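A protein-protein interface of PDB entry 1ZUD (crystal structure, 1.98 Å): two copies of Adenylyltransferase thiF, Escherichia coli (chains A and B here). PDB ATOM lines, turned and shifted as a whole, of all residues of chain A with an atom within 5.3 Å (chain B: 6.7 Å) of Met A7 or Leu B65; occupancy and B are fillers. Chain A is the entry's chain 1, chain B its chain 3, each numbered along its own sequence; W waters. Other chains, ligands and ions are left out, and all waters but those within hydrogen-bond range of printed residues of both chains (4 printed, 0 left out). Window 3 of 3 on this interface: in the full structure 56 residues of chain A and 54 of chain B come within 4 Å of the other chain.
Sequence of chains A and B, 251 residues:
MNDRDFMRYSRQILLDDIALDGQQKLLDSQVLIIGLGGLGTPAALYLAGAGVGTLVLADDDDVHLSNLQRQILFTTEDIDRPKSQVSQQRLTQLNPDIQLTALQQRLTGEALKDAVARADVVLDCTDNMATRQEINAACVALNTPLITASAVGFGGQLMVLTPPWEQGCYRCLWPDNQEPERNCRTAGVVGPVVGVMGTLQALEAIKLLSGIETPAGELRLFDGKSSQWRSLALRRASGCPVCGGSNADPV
No position is printed for both chains.
Water W1 lies within hydrogen-bond range of the backbone carbonyl oxygen of Arg A8 (2.5 Å), the backbone NH of Gln B69 (2.6 Å), the backbone carbonyl oxygen of Leu B65 (2.8 Å) and the backbone NH of Leu B68 (3.3 Å). Water W2 lies within hydrogen-bond range of the backbone NH of Arg A11 (2.8 Å), the backbone carbonyl oxygen of Arg A8 (2.9 Å), the backbone carbonyl oxygen of Ser B66 (2.9 Å) and the backbone NH of Ser A10 (3.4 Å). Water W4 lies within hydrogen-bond range of the guanidinium group of Arg A8 (2.9 Å) and the backbone NH of Gln B69 (3.4 Å). Water W3 bridges N of Ser B66 (3.2 Å) and SD of Met A7 (3.6 Å).
Of chain B, only Leu B65 and Ser B66 come within 4 Å of Met A7. Of the printed residues of chain B, Arg A8 touches Leu B65 (3.6 Å), Ser B66 (3.99 Å), Leu B68 (3.9 Å), Gln B69 (3.9 Å) and Thr B76 (3.1 Å). Printed residues of chain B within 4 Å of Ser A10: Ser B66 (3.5 Å). Of the printed residues of chain B, Arg A11 touches Gln B69 (3.8 Å). Of chain A, only Met A7 and Arg A8 come within 4 Å of Leu B65. Of the printed residues of chain A, Ser B66 touches Met A7, Arg A8 and Ser A10. Of the printed residues of chain A, Leu B68 touches Arg A8. The nearest residue of chain B that does not touch Met A7 is Asn B67 (6.1 Å).
O of Met A7 is in hydrogen-bond range of OG of Ser A10 (2.7 Å).
Of the 10 printed residues of chain B, 5 touch a printed residue of chain A. Printed residues of chain B that touch a printed residue of chain A: Leu B65, Ser B66, Leu B68, Gln B69 and Thr B76. Hydrophobic or aromatic side chains of chain B within 4 Å of the printed part of chain A: Leu B65 and Leu B68. Among the printed residues, no Asp or Glu carboxylate lies within 4 Å of a Lys or Arg side-chain nitrogen of the other chain.
NH2 of Arg A8 lies within hydrogen-bond range of OG1 of Thr B76 (3.1 Å).
Met A7 touches Leu B65 (CG to CD2, 3.95 Å). CE of Met A7 touches CB of Ser B66, 3.0 Å away. Leu B65 touches Arg A8 (CD1 to NH2, 3.6 Å). Ser B66 touches Arg A8 (CA to O, 3.99 Å). Arg A8 touches Leu B68. Arg A8 touches Gln B69. Ser B66 touches Ser A10 (CB to OG, 3.5 Å). CB of Arg A11 touches OE1 of Gln B69, at 3.8 Å.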
ATOM      1  N   ASP A   3      30.297  16.390  24.846  1.00  0.00           N
ATOM      2  CA  ASP A   3      29.475  17.292  24.069  1.00  0.00           C
ATOM      3  C   ASP A   3      29.025  18.546  24.816  1.00  0.00           C
ATOM      4  O   ASP A   3      28.997  19.633  24.235  1.00  0.00           O
ATOM      5  CB  ASP A   3      28.230  16.579  23.539  1.00  0.00           C
ATOM      6  CG  ASP A   3      28.567  15.336  22.728  1.00  0.00           C
ATOM      7  OD1 ASP A   3      27.641  14.793  22.089  1.00  0.00           O
ATOM      8  OD2 ASP A   3      29.746  14.896  22.729  1.00  0.00           O
ATOM      9  N   ARG A   4      28.648  18.392  26.082  1.00  0.00           N
ATOM     10  CA  ARG A   4      28.203  19.532  26.864  1.00  0.00           C
ATOM     11  C   ARG A   4      29.345  20.587  27.003  1.00  0.00           C
ATOM     12  O   ARG A   4      29.096  21.774  26.848  1.00  0.00           O
ATOM     13  CB  ARG A   4      27.680  19.075  28.242  1.00  0.00           C
ATOM     14  CG  ARG A   4      27.203  20.259  29.116  1.00  0.00           C
ATOM     15  CD  ARG A   4      26.115  19.938  30.146  1.00  0.00           C
ATOM     16  NE  ARG A   4      26.384  18.858  31.118  1.00  0.00           N
ATOM     17  CZ  ARG A   4      27.582  18.433  31.518  1.00  0.00           C
ATOM     18  NH1 ARG A   4      28.690  18.976  31.036  1.00  0.00           N
ATOM     19  NH2 ARG A   4      27.669  17.468  32.429  1.00  0.00           N
ATOM     20  N   ASP A   5      30.573  20.161  27.299  1.00  0.00           N
ATOM     21  CA  ASP A   5      31.697  21.113  27.384  1.00  0.00           C
ATOM     22  C   ASP A   5      31.967  21.773  26.019  1.00  0.00           C
ATOM     23  O   ASP A   5      32.260  22.972  25.935  1.00  0.00           O
ATOM     24  CB  ASP A   5      32.983  20.429  27.854  1.00  0.00           C
ATOM     25  CG  ASP A   5      32.881  19.923  29.322  1.00  0.00           C
ATOM     26  OD1 ASP A   5      32.071  20.470  30.116  1.00  0.00           O
ATOM     27  OD2 ASP A   5      33.625  18.988  29.683  1.00  0.00           O
ATOM     28  N   PHE A   6      31.864  21.001  24.951  1.00  0.00           N
ATOM     29  CA  PHE A   6      32.095  21.570  23.611  1.00  0.00           C
ATOM     30  C   PHE A   6      31.136  22.731  23.321  1.00  0.00           C
ATOM     31  O   PHE A   6      31.558  23.836  22.896  1.00  0.00           O
ATOM     32  CB  PHE A   6      31.944  20.490  22.519  1.00  0.00           C
ATOM     33  CG  PHE A   6      32.378  20.961  21.161  1.00  0.00           C
ATOM     34  CD1 PHE A   6      31.435  21.318  20.197  1.00  0.00           C
ATOM     35  CD2 PHE A   6      33.738  21.126  20.873  1.00  0.00           C
ATOM     36  CE1 PHE A   6      31.847  21.834  18.972  1.00  0.00           C
ATOM     37  CE2 PHE A   6      34.167  21.653  19.627  1.00  0.00           C
ATOM     38  CZ  PHE A   6      33.223  22.004  18.687  1.00  0.00           C
ATOM     39  N   MET A   7      29.842  22.511  23.520  1.00  0.00           N
ATOM     40  CA  MET A   7      28.886  23.618  23.303  1.00  0.00           C
ATOM     41  C   MET A   7      29.123  24.804  24.252  1.00  0.00           C
ATOM     42  O   MET A   7      29.131  25.992  23.832  1.00  0.00           O
ATOM     43  CB  MET A   7      27.449  23.172  23.511  1.00  0.00           C
ATOM     44  CG  MET A   7      26.442  24.320  23.238  1.00  0.00           C
ATOM     45  SD  MET A   7      26.436  24.836  21.456  1.00  0.00           S
ATOM     46  CE  MET A   7      27.055  26.410  21.507  1.00  0.00           C
ATOM     47  N   ARG A   8      29.269  24.482  25.541  1.00  0.00           N
ATOM     48  CA  ARG A   8      29.511  25.515  26.555  1.00  0.00           C
ATOM     49  C   ARG A   8      30.702  26.415  26.208  1.00  0.00           C
ATOM     50  O   ARG A   8      30.590  27.626  26.376  1.00  0.00           O
ATOM     51  CB  ARG A   8      29.776  24.912  27.960  1.00  0.00           C
ATOM     52  CG  ARG A   8      30.222  25.971  28.972  1.00  0.00           C
ATOM     53  CD  ARG A   8      30.465  25.321  30.381  1.00  0.00           C
ATOM     54  NE  ARG A   8      29.214  24.923  31.000  1.00  0.00           N
ATOM     55  CZ  ARG A   8      28.425  25.735  31.709  1.00  0.00           C
ATOM     56  NH1 ARG A   8      28.757  27.004  31.904  1.00  0.00           N
ATOM     57  NH2 ARG A   8      27.290  25.271  32.227  1.00  0.00           N
ATOM     58  N   TYR A   9      31.830  25.821  25.764  1.00  0.00           N
ATOM     59  CA  TYR A   9      33.032  26.593  25.449  1.00  0.00           C
ATOM     60  C   TYR A   9      33.244  26.891  23.978  1.00  0.00           C
ATOM     61  O   TYR A   9      34.308  27.359  23.614  1.00  0.00           O
ATOM     62  CB  TYR A   9      34.287  25.862  25.974  1.00  0.00           C
ATOM     63  CG  TYR A   9      34.145  25.517  27.435  1.00  0.00           C
ATOM     64  CD1 TYR A   9      34.183  24.196  27.850  1.00  0.00           C
ATOM     65  CD2 TYR A   9      33.941  26.519  28.398  1.00  0.00           C
ATOM     66  CE1 TYR A   9      34.026  23.852  29.213  1.00  0.00           C
ATOM     67  CE2 TYR A   9      33.764  26.195  29.763  1.00  0.00           C
ATOM     68  CZ  TYR A   9      33.819  24.838  30.145  1.00  0.00           C
ATOM     69  OH  TYR A   9      33.682  24.474  31.460  1.00  0.00           O
ATOM     70  N   SER A  10      32.214  26.681  23.181  1.00  0.00           N
ATOM     71  CA  SER A  10      32.301  26.822  21.744  1.00  0.00           C
ATOM     72  C   SER A  10      32.821  28.179  21.281  1.00  0.00           C
ATOM     73  O   SER A  10      33.662  28.214  20.377  1.00  0.00           O
ATOM     74  CB  SER A  10      30.934  26.530  21.100  1.00  0.00           C
ATOM     75  OG  SER A  10      29.934  27.384  21.631  1.00  0.00           O
ATOM     76  N   ARG A  11      32.392  29.275  21.910  1.00  0.00           N
ATOM     77  CA  ARG A  11      32.856  30.581  21.417  1.00  0.00           C
ATOM     78  C   ARG A  11      34.331  30.853  21.616  1.00  0.00           C
ATOM     79  O   ARG A  11      34.896  31.705  20.916  1.00  0.00           O
ATOM     80  CB  ARG A  11      32.013  31.711  22.025  1.00  0.00           C
ATOM     81  CG  ARG A  11      30.525  31.593  21.727  1.00  0.00           C
ATOM     82  CD  ARG A  11      30.269  30.943  20.363  1.00  0.00           C
ATOM     83  NE  ARG A  11      29.020  31.384  19.753  1.00  0.00           N
ATOM     84  CZ  ARG A  11      28.819  32.599  19.242  1.00  0.00           C
ATOM     85  NH1 ARG A  11      29.790  33.506  19.262  1.00  0.00           N
ATOM     86  NH2 ARG A  11      27.644  32.912  18.707  1.00  0.00           N
ATOM     87  N   VAL B  63      18.471  33.110  26.788  1.00  0.00           N
ATOM     88  CA  VAL B  63      19.765  32.606  27.203  1.00  0.00           C
ATOM     89  C   VAL B  63      20.082  31.245  26.554  1.00  0.00           C
ATOM     90  O   VAL B  63      19.227  30.357  26.474  1.00  0.00           O
ATOM     91  CB  VAL B  63      19.825  32.498  28.743  1.00  0.00           C
ATOM     92  CG1 VAL B  63      21.197  31.953  29.168  1.00  0.00           C
ATOM     93  CG2 VAL B  63      19.516  33.937  29.380  1.00  0.00           C
ATOM     94  N   HIS B  64      21.322  31.069  26.098  1.00  0.00           N
ATOM     95  CA  HIS B  64      21.736  29.796  25.483  1.00  0.00           C
ATOM     96  C   HIS B  64      22.939  29.350  26.277  1.00  0.00           C
ATOM     97  O   HIS B  64      23.663  30.194  26.802  1.00  0.00           O
ATOM     98  CB  HIS B  64      22.115  30.005  24.013  1.00  0.00           C
ATOM     99  CG  HIS B  64      21.007  30.585  23.188  1.00  0.00           C
ATOM    100  ND1 HIS B  64      19.781  29.968  23.044  1.00  0.00           N
ATOM    101  CD2 HIS B  64      20.915  31.761  22.518  1.00  0.00           C
ATOM    102  CE1 HIS B  64      18.980  30.741  22.330  1.00  0.00           C
ATOM    103  NE2 HIS B  64      19.645  31.836  22.001  1.00  0.00           N
ATOM    104  N   LEU B  65      23.219  28.040  26.290  1.00  0.00           N
ATOM    105  CA  LEU B  65      24.339  27.533  27.069  1.00  0.00           C
ATOM    106  C   LEU B  65      25.670  28.165  26.651  1.00  0.00           C
ATOM    107  O   LEU B  65      26.506  28.464  27.500  1.00  0.00           O
ATOM    108  CB  LEU B  65      24.422  25.989  26.926  1.00  0.00           C
ATOM    109  CG  LEU B  65      25.697  25.321  27.423  1.00  0.00           C
ATOM    110  CD1 LEU B  65      25.845  25.566  28.968  1.00  0.00           C
ATOM    111  CD2 LEU B  65      25.629  23.823  27.076  1.00  0.00           C
ATOM    112  N   SER B  66      25.870  28.345  25.344  1.00  0.00           N
ATOM    113  CA  SER B  66      27.135  28.915  24.863  1.00  0.00           C
ATOM    114  C   SER B  66      27.354  30.396  25.264  1.00  0.00           C
ATOM    115  O   SER B  66      28.449  30.931  25.118  1.00  0.00           O
ATOM    116  CB  SER B  66      27.230  28.768  23.349  1.00  0.00           C
ATOM    117  OG  SER B  66      26.315  29.648  22.749  1.00  0.00           O
ATOM    118  N   ASN B  67      26.315  31.048  25.756  1.00  0.00           N
ATOM    119  CA  ASN B  67      26.403  32.431  26.257  1.00  0.00           C
ATOM    120  C   ASN B  67      27.200  32.563  27.553  1.00  0.00           C
ATOM    121  O   ASN B  67      27.850  33.576  27.802  1.00  0.00           O
ATOM    122  CB  ASN B  67      25.011  32.962  26.649  1.00  0.00           C
ATOM    123  CG  ASN B  67      24.067  33.132  25.472  1.00  0.00           C
ATOM    124  OD1 ASN B  67      22.889  33.379  25.691  1.00  0.00           O
ATOM    125  ND2 ASN B  67      24.578  33.018  24.230  1.00  0.00           N
ATOM    126  N   LEU B  68      27.108  31.537  28.400  1.00  0.00           N
ATOM    127  CA  LEU B  68      27.669  31.601  29.718  1.00  0.00           C
ATOM    128  C   LEU B  68      29.158  31.848  29.782  1.00  0.00           C
ATOM    129  O   LEU B  68      29.624  32.397  30.762  1.00  0.00           O
ATOM    130  CB  LEU B  68      27.270  30.330  30.522  1.00  0.00           C
ATOM    131  CG  LEU B  68      25.722  30.077  30.536  1.00  0.00           C
ATOM    132  CD1 LEU B  68      25.325  28.899  31.545  1.00  0.00           C
ATOM    133  CD2 LEU B  68      24.966  31.370  30.989  1.00  0.00           C
ATOM    134  N   GLN B  69      29.896  31.493  28.741  1.00  0.00           N
ATOM    135  CA  GLN B  69      31.334  31.717  28.757  1.00  0.00           C
ATOM    136  C   GLN B  69      31.661  33.216  28.860  1.00  0.00           C
ATOM    137  O   GLN B  69      32.788  33.583  29.210  1.00  0.00           O
ATOM    138  CB  GLN B  69      31.924  31.101  27.475  1.00  0.00           C
ATOM    139  CG  GLN B  69      33.350  31.419  27.163  1.00  0.00           C
ATOM    140  CD  GLN B  69      33.413  32.486  26.033  1.00  0.00           C
ATOM    141  OE1 GLN B  69      32.376  32.987  25.601  1.00  0.00           O
ATOM    142  NE2 GLN B  69      34.604  32.809  25.572  1.00  0.00           N
ATOM    143  N   THR B  76      23.146  28.617  34.438  1.00  0.00           N
ATOM    144  CA  THR B  76      22.614  27.464  33.750  1.00  0.00           C
ATOM    145  C   THR B  76      21.104  27.376  33.965  1.00  0.00           C
ATOM    146  O   THR B  76      20.387  26.903  33.092  1.00  0.00           O
ATOM    147  CB  THR B  76      23.345  26.151  34.241  1.00  0.00           C
ATOM    148  OG1 THR B  76      24.689  26.158  33.757  1.00  0.00           O
ATOM    149  CG2 THR B  76      22.711  24.910  33.680  1.00  0.00           C
ATOM    150  N   ILE B  79      18.839  29.113  31.206  1.00  0.00           N
ATOM    151  CA  ILE B  79      18.805  28.744  29.798  1.00  0.00           C
ATOM    152  C   ILE B  79      17.376  28.671  29.235  1.00  0.00           C
ATOM    153  O   ILE B  79      16.473  28.169  29.886  1.00  0.00           O
ATOM    154  CB  ILE B  79      19.617  27.446  29.575  1.00  0.00           C
ATOM    155  CG1 ILE B  79      21.108  27.774  29.757  1.00  0.00           C
ATOM    156  CG2 ILE B  79      19.234  26.765  28.244  1.00  0.00           C
ATOM    157  CD1 ILE B  79      21.999  26.539  30.052  1.00  0.00           C
ATOM    158  N   ASP B  80      17.190  29.236  28.034  1.00  0.00           N
ATOM    159  CA  ASP B  80      15.911  29.300  27.340  1.00  0.00           C
ATOM    160  C   ASP B  80      14.971  30.412  27.794  1.00  0.00           C
ATOM    161  O   ASP B  80      13.932  30.621  27.200  1.00  0.00           O
ATOM    162  CB  ASP B  80      15.160  27.950  27.354  1.00  0.00           C
ATOM    163  CG  ASP B  80      15.883  26.859  26.574  1.00  0.00           C
ATOM    164  OD1 ASP B  80      16.624  27.176  25.615  1.00  0.00           O
ATOM    165  OD2 ASP B  80      15.699  25.669  26.919  1.00  0.00           O
HETATM  166  O   HOH W   1      29.235  29.052  27.981  1.00  0.00           O
HETATM  167  O   HOH W   2      30.849  29.564  24.236  1.00  0.00           O
HETATM  168  O   HOH W   3      24.083  27.169  22.971  1.00  0.00           O
HETATM  169  O   HOH W   4      30.624  28.694  30.548  1.00  0.00           O
